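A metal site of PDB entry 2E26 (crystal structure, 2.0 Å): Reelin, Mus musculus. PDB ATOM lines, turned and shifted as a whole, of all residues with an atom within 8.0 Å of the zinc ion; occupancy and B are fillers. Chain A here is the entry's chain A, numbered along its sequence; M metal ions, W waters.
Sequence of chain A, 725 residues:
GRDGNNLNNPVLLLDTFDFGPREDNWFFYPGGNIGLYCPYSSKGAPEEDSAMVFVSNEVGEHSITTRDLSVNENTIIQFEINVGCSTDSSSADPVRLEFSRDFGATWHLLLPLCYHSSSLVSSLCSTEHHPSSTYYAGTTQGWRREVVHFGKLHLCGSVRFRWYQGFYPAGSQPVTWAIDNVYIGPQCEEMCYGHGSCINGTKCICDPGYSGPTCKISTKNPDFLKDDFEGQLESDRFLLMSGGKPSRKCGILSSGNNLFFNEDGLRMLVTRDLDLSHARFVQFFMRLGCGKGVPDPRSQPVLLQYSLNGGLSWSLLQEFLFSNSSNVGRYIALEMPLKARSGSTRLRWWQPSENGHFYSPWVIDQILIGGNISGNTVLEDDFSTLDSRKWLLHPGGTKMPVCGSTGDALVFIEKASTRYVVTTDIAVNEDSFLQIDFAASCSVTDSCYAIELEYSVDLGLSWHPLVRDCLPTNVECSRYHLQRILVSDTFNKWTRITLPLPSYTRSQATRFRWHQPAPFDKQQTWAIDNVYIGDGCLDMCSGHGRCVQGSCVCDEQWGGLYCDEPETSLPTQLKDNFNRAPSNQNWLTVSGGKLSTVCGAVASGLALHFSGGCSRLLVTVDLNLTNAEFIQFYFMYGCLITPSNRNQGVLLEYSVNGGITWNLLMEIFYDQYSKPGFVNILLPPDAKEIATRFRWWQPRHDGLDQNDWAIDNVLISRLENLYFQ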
ATOM      1  N   ARG A 419      10.510  -8.658  21.037  1.00  0.00           N
ATOM      2  CA  ARG A 419       9.704  -9.272  22.072  1.00  0.00           C
ATOM      3  C   ARG A 419       9.224 -10.632  21.612  1.00  0.00           C
ATOM      4  O   ARG A 419       8.348 -10.738  20.746  1.00  0.00           O
ATOM      5  CB  ARG A 419       8.494  -8.396  22.423  1.00  0.00           C
ATOM      6  CG  ARG A 419       8.815  -7.099  23.142  1.00  0.00           C
ATOM      7  CD  ARG A 419       7.554  -6.272  23.288  1.00  0.00           C
ATOM      8  NE  ARG A 419       7.750  -5.085  24.105  1.00  0.00           N
ATOM      9  CZ  ARG A 419       6.931  -4.039  24.096  1.00  0.00           C
ATOM     10  NH1 ARG A 419       5.865  -4.028  23.306  1.00  0.00           N
ATOM     11  NH2 ARG A 419       7.178  -2.989  24.879  1.00  0.00           N
ATOM     12  N   TYR A 420       9.806 -11.680  22.189  1.00  0.00           N
ATOM     13  CA  TYR A 420       9.287 -13.023  22.027  1.00  0.00           C
ATOM     14  C   TYR A 420       9.702 -13.940  23.179  1.00  0.00           C
ATOM     15  O   TYR A 420      10.545 -13.584  23.984  1.00  0.00           O
ATOM     16  CB  TYR A 420       9.680 -13.625  20.664  1.00  0.00           C
ATOM     17  CG  TYR A 420      11.145 -13.889  20.366  1.00  0.00           C
ATOM     18  CD1 TYR A 420      11.809 -14.979  20.942  1.00  0.00           C
ATOM     19  CD2 TYR A 420      11.836 -13.108  19.444  1.00  0.00           C
ATOM     20  CE1 TYR A 420      13.145 -15.248  20.642  1.00  0.00           C
ATOM     21  CE2 TYR A 420      13.180 -13.377  19.131  1.00  0.00           C
ATOM     22  CZ  TYR A 420      13.809 -14.448  19.744  1.00  0.00           C
ATOM     23  OH  TYR A 420      15.117 -14.720  19.435  1.00  0.00           O
ATOM     24  N   ILE A 451      -0.465 -10.753  18.854  1.00  0.00           N
ATOM     25  CA  ILE A 451       0.780 -11.440  19.152  1.00  0.00           C
ATOM     26  C   ILE A 451       0.673 -12.790  18.504  1.00  0.00           C
ATOM     27  O   ILE A 451      -0.332 -13.491  18.692  1.00  0.00           O
ATOM     28  CB  ILE A 451       0.990 -11.593  20.682  1.00  0.00           C
ATOM     29  CG1 ILE A 451       0.991 -10.225  21.381  1.00  0.00           C
ATOM     30  CG2 ILE A 451       2.250 -12.427  20.989  1.00  0.00           C
ATOM     31  CD1 ILE A 451       1.828  -9.119  20.744  1.00  0.00           C
ATOM     32  N   GLU A 452       1.695 -13.168  17.742  1.00  0.00           N
ATOM     33  CA  GLU A 452       1.700 -14.399  16.980  1.00  0.00           C
ATOM     34  C   GLU A 452       2.023 -15.580  17.887  1.00  0.00           C
ATOM     35  O   GLU A 452       2.899 -15.480  18.745  1.00  0.00           O
ATOM     36  CB  GLU A 452       2.719 -14.339  15.835  1.00  0.00           C
ATOM     37  CG  GLU A 452       2.432 -13.247  14.793  1.00  0.00           C
ATOM     38  CD  GLU A 452       3.552 -13.079  13.742  1.00  0.00           C
ATOM     39  OE1 GLU A 452       3.219 -12.738  12.583  1.00  0.00           O
ATOM     40  OE2 GLU A 452       4.749 -13.282  14.068  1.00  0.00           O
ATOM     41  N   LEU A 453       1.314 -16.684  17.701  1.00  0.00           N
ATOM     42  CA  LEU A 453       1.671 -17.925  18.373  1.00  0.00           C
ATOM     43  C   LEU A 453       2.113 -18.932  17.321  1.00  0.00           C
ATOM     44  O   LEU A 453       1.387 -19.197  16.348  1.00  0.00           O
ATOM     45  CB  LEU A 453       0.515 -18.445  19.222  1.00  0.00           C
ATOM     46  CG  LEU A 453       0.599 -19.781  19.977  1.00  0.00           C
ATOM     47  CD1 LEU A 453       1.886 -19.931  20.786  1.00  0.00           C
ATOM     48  CD2 LEU A 453      -0.628 -19.914  20.881  1.00  0.00           C
ATOM     49  N   GLU A 454       3.303 -19.470  17.527  1.00  0.00           N
ATOM     50  CA  GLU A 454       4.020 -20.266  16.533  1.00  0.00           C
ATOM     51  C   GLU A 454       4.559 -21.550  17.141  1.00  0.00           C
ATOM     52  O   GLU A 454       4.664 -21.648  18.369  1.00  0.00           O
ATOM     53  CB  GLU A 454       5.172 -19.425  15.979  1.00  0.00           C
ATOM     54  CG  GLU A 454       4.672 -18.207  15.221  1.00  0.00           C
ATOM     55  CD  GLU A 454       5.698 -17.125  15.053  1.00  0.00           C
ATOM     56  OE1 GLU A 454       6.824 -17.217  15.607  1.00  0.00           O
ATOM     57  OE2 GLU A 454       5.374 -16.148  14.368  1.00  0.00           O
ATOM     58  N   TRP A 463       9.901 -21.488  12.220  1.00  0.00           N
ATOM     59  CA  TRP A 463       8.720 -21.285  13.052  1.00  0.00           C
ATOM     60  C   TRP A 463       7.523 -21.103  12.124  1.00  0.00           C
ATOM     61  O   TRP A 463       7.629 -20.458  11.063  1.00  0.00           O
ATOM     62  CB  TRP A 463       8.897 -20.054  13.948  1.00  0.00           C
ATOM     63  CG  TRP A 463       9.906 -20.238  15.027  1.00  0.00           C
ATOM     64  CD1 TRP A 463      11.210 -19.811  15.011  1.00  0.00           C
ATOM     65  CD2 TRP A 463       9.705 -20.890  16.286  1.00  0.00           C
ATOM     66  NE1 TRP A 463      11.833 -20.163  16.188  1.00  0.00           N
ATOM     67  CE2 TRP A 463      10.935 -20.825  16.986  1.00  0.00           C
ATOM     68  CE3 TRP A 463       8.620 -21.537  16.880  1.00  0.00           C
ATOM     69  CZ2 TRP A 463      11.104 -21.379  18.261  1.00  0.00           C
ATOM     70  CZ3 TRP A 463       8.789 -22.095  18.147  1.00  0.00           C
ATOM     71  CH2 TRP A 463      10.021 -22.012  18.824  1.00  0.00           C
ATOM     72  N   HIS A 464       6.391 -21.686  12.491  1.00  0.00           N
ATOM     73  CA  HIS A 464       5.191 -21.672  11.669  1.00  0.00           C
ATOM     74  C   HIS A 464       3.993 -21.336  12.548  1.00  0.00           C
ATOM     75  O   HIS A 464       3.950 -21.753  13.712  1.00  0.00           O
ATOM     76  CB  HIS A 464       4.997 -23.048  11.018  1.00  0.00           C
ATOM     77  CG  HIS A 464       6.190 -23.493  10.244  1.00  0.00           C
ATOM     78  ND1 HIS A 464       7.171 -24.309  10.787  1.00  0.00           N
ATOM     79  CD2 HIS A 464       6.600 -23.202   8.980  1.00  0.00           C
ATOM     80  CE1 HIS A 464       8.111 -24.515   9.885  1.00  0.00           C
ATOM     81  NE2 HIS A 464       7.793 -23.853   8.784  1.00  0.00           N
ATOM     82  N   PRO A 465       3.015 -20.573  12.015  1.00  0.00           N
ATOM     83  CA  PRO A 465       1.876 -20.217  12.855  1.00  0.00           C
ATOM     84  C   PRO A 465       1.156 -21.462  13.373  1.00  0.00           C
ATOM     85  O   PRO A 465       0.945 -22.418  12.613  1.00  0.00           O
ATOM     86  CB  PRO A 465       0.964 -19.422  11.907  1.00  0.00           C
ATOM     87  CG  PRO A 465       1.467 -19.680  10.535  1.00  0.00           C
ATOM     88  CD  PRO A 465       2.916 -20.033  10.650  1.00  0.00           C
ATOM     89  N   LEU A 482      -1.887 -17.527   8.469  1.00  0.00           N
ATOM     90  CA  LEU A 482      -2.151 -17.515   9.903  1.00  0.00           C
ATOM     91  C   LEU A 482      -3.445 -16.778  10.285  1.00  0.00           C
ATOM     92  O   LEU A 482      -3.881 -15.859   9.583  1.00  0.00           O
ATOM     93  CB  LEU A 482      -0.954 -16.952  10.681  1.00  0.00           C
ATOM     94  CG  LEU A 482      -0.561 -15.459  10.765  1.00  0.00           C
ATOM     95  CD1 LEU A 482       0.389 -15.271  11.932  1.00  0.00           C
ATOM     96  CD2 LEU A 482       0.069 -14.938   9.476  1.00  0.00           C
ATOM     97  N   ARG A 513       6.490 -20.598  20.375  1.00  0.00           N
ATOM     98  CA  ARG A 513       6.963 -19.230  20.475  1.00  0.00           C
ATOM     99  C   ARG A 513       5.790 -18.254  20.418  1.00  0.00           C
ATOM    100  O   ARG A 513       4.920 -18.367  19.556  1.00  0.00           O
ATOM    101  CB  ARG A 513       7.997 -18.912  19.381  1.00  0.00           C
ATOM    102  CG  ARG A 513       8.617 -17.499  19.470  1.00  0.00           C
ATOM    103  CD  ARG A 513       9.778 -17.257  18.477  1.00  0.00           C
ATOM    104  NE  ARG A 513       9.315 -17.054  17.091  1.00  0.00           N
ATOM    105  CZ  ARG A 513      10.089 -16.613  16.096  1.00  0.00           C
ATOM    106  NH1 ARG A 513      11.364 -16.311  16.302  1.00  0.00           N
ATOM    107  NH2 ARG A 513       9.577 -16.455  14.870  1.00  0.00           N
ATOM    108  N   TRP A 514       5.755 -17.314  21.353  1.00  0.00           N
ATOM    109  CA  TRP A 514       4.906 -16.146  21.268  1.00  0.00           C
ATOM    110  C   TRP A 514       5.776 -15.047  20.717  1.00  0.00           C
ATOM    111  O   TRP A 514       6.819 -14.731  21.279  1.00  0.00           O
ATOM    112  CB  TRP A 514       4.367 -15.740  22.643  1.00  0.00           C
ATOM    113  CG  TRP A 514       3.327 -16.671  23.166  1.00  0.00           C
ATOM    114  CD1 TRP A 514       1.975 -16.466  23.177  1.00  0.00           C
ATOM    115  CD2 TRP A 514       3.546 -17.969  23.738  1.00  0.00           C
ATOM    116  NE1 TRP A 514       1.340 -17.558  23.737  1.00  0.00           N
ATOM    117  CE2 TRP A 514       2.278 -18.487  24.082  1.00  0.00           C
ATOM    118  CE3 TRP A 514       4.685 -18.732  24.006  1.00  0.00           C
ATOM    119  CZ2 TRP A 514       2.122 -19.753  24.684  1.00  0.00           C
ATOM    120  CZ3 TRP A 514       4.531 -19.986  24.601  1.00  0.00           C
ATOM    121  CH2 TRP A 514       3.258 -20.485  24.932  1.00  0.00           C
ATOM    122  N   HIS A 515       5.357 -14.479  19.596  1.00  0.00           N
ATOM    123  CA  HIS A 515       6.202 -13.536  18.873  1.00  0.00           C
ATOM    124  C   HIS A 515       5.445 -12.254  18.547  1.00  0.00           C
ATOM    125  O   HIS A 515       4.363 -12.309  17.953  1.00  0.00           O
ATOM    126  CB  HIS A 515       6.709 -14.199  17.579  1.00  0.00           C
ATOM    127  CG  HIS A 515       7.707 -13.368  16.824  1.00  0.00           C
ATOM    128  ND1 HIS A 515       7.811 -13.409  15.451  1.00  0.00           N
ATOM    129  CD2 HIS A 515       8.634 -12.483  17.257  1.00  0.00           C
ATOM    130  CE1 HIS A 515       8.767 -12.583  15.067  1.00  0.00           C
ATOM    131  NE2 HIS A 515       9.286 -12.008  16.138  1.00  0.00           N
ATOM    132  N   GLN A 516       6.006 -11.107  18.948  1.00  0.00           N
ATOM    133  CA  GLN A 516       5.495  -9.801  18.514  1.00  0.00           C
ATOM    134  C   GLN A 516       6.344  -9.283  17.348  1.00  0.00           C
ATOM    135  O   GLN A 516       7.463  -8.810  17.559  1.00  0.00           O
ATOM    136  CB  GLN A 516       5.443  -8.783  19.660  1.00  0.00           C
ATOM    137  CG  GLN A 516       4.801  -7.423  19.221  1.00  0.00           C
ATOM    138  CD  GLN A 516       4.448  -6.506  20.385  1.00  0.00           C
ATOM    139  OE1 GLN A 516       5.113  -6.506  21.421  1.00  0.00           O
ATOM    140  NE2 GLN A 516       3.402  -5.711  20.224  1.00  0.00           N
ATOM    141  N   PRO A 517       5.830  -9.373  16.114  1.00  0.00           N
ATOM    142  CA  PRO A 517       6.717  -9.042  15.005  1.00  0.00           C
ATOM    143  C   PRO A 517       7.075  -7.552  14.986  1.00  0.00           C
ATOM    144  O   PRO A 517       6.233  -6.701  15.278  1.00  0.00           O
ATOM    145  CB  PRO A 517       5.917  -9.460  13.764  1.00  0.00           C
ATOM    146  CG  PRO A 517       4.492  -9.433  14.185  1.00  0.00           C
ATOM    147  CD  PRO A 517       4.456  -9.717  15.666  1.00  0.00           C
ATOM    148  N   ALA A 518       8.342  -7.264  14.692  1.00  0.00           N
ATOM    149  CA  ALA A 518       8.807  -5.881  14.523  1.00  0.00           C
ATOM    150  C   ALA A 518       8.371  -5.385  13.154  1.00  0.00           C
ATOM    151  O   ALA A 518       8.320  -6.177  12.200  1.00  0.00           O
ATOM    152  CB  ALA A 518      10.324  -5.817  14.645  1.00  0.00           C
HETATM  153 ZN    ZN M   1       6.553 -14.585  14.068  1.00  0.00          ZN
HETATM  154  O   HOH W   1       7.924 -15.568  12.395  1.00  0.00           O
HETATM  155  O   HOH W   2       6.206 -12.981  11.783  1.00  0.00           O
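OE1 of Glu 454 is in salt-bridge range of NE of Arg 513 (2.9 Å).
Residues that only touch the zinc ion: Arg 513 (3.6 Å).
Within 4 Å of the zinc ion: Glu 452, Glu 454, Arg 513 and His 515.
The zinc ion is bound by OE2 of Glu 454 (2.0 Å), ND1 of His 515 (2.2 Å), OE2 of Glu 452 (2.2 Å) and water W1 (2.4 Å).
Slightly farther from the zinc ion lies water W2 (2.8 Å).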
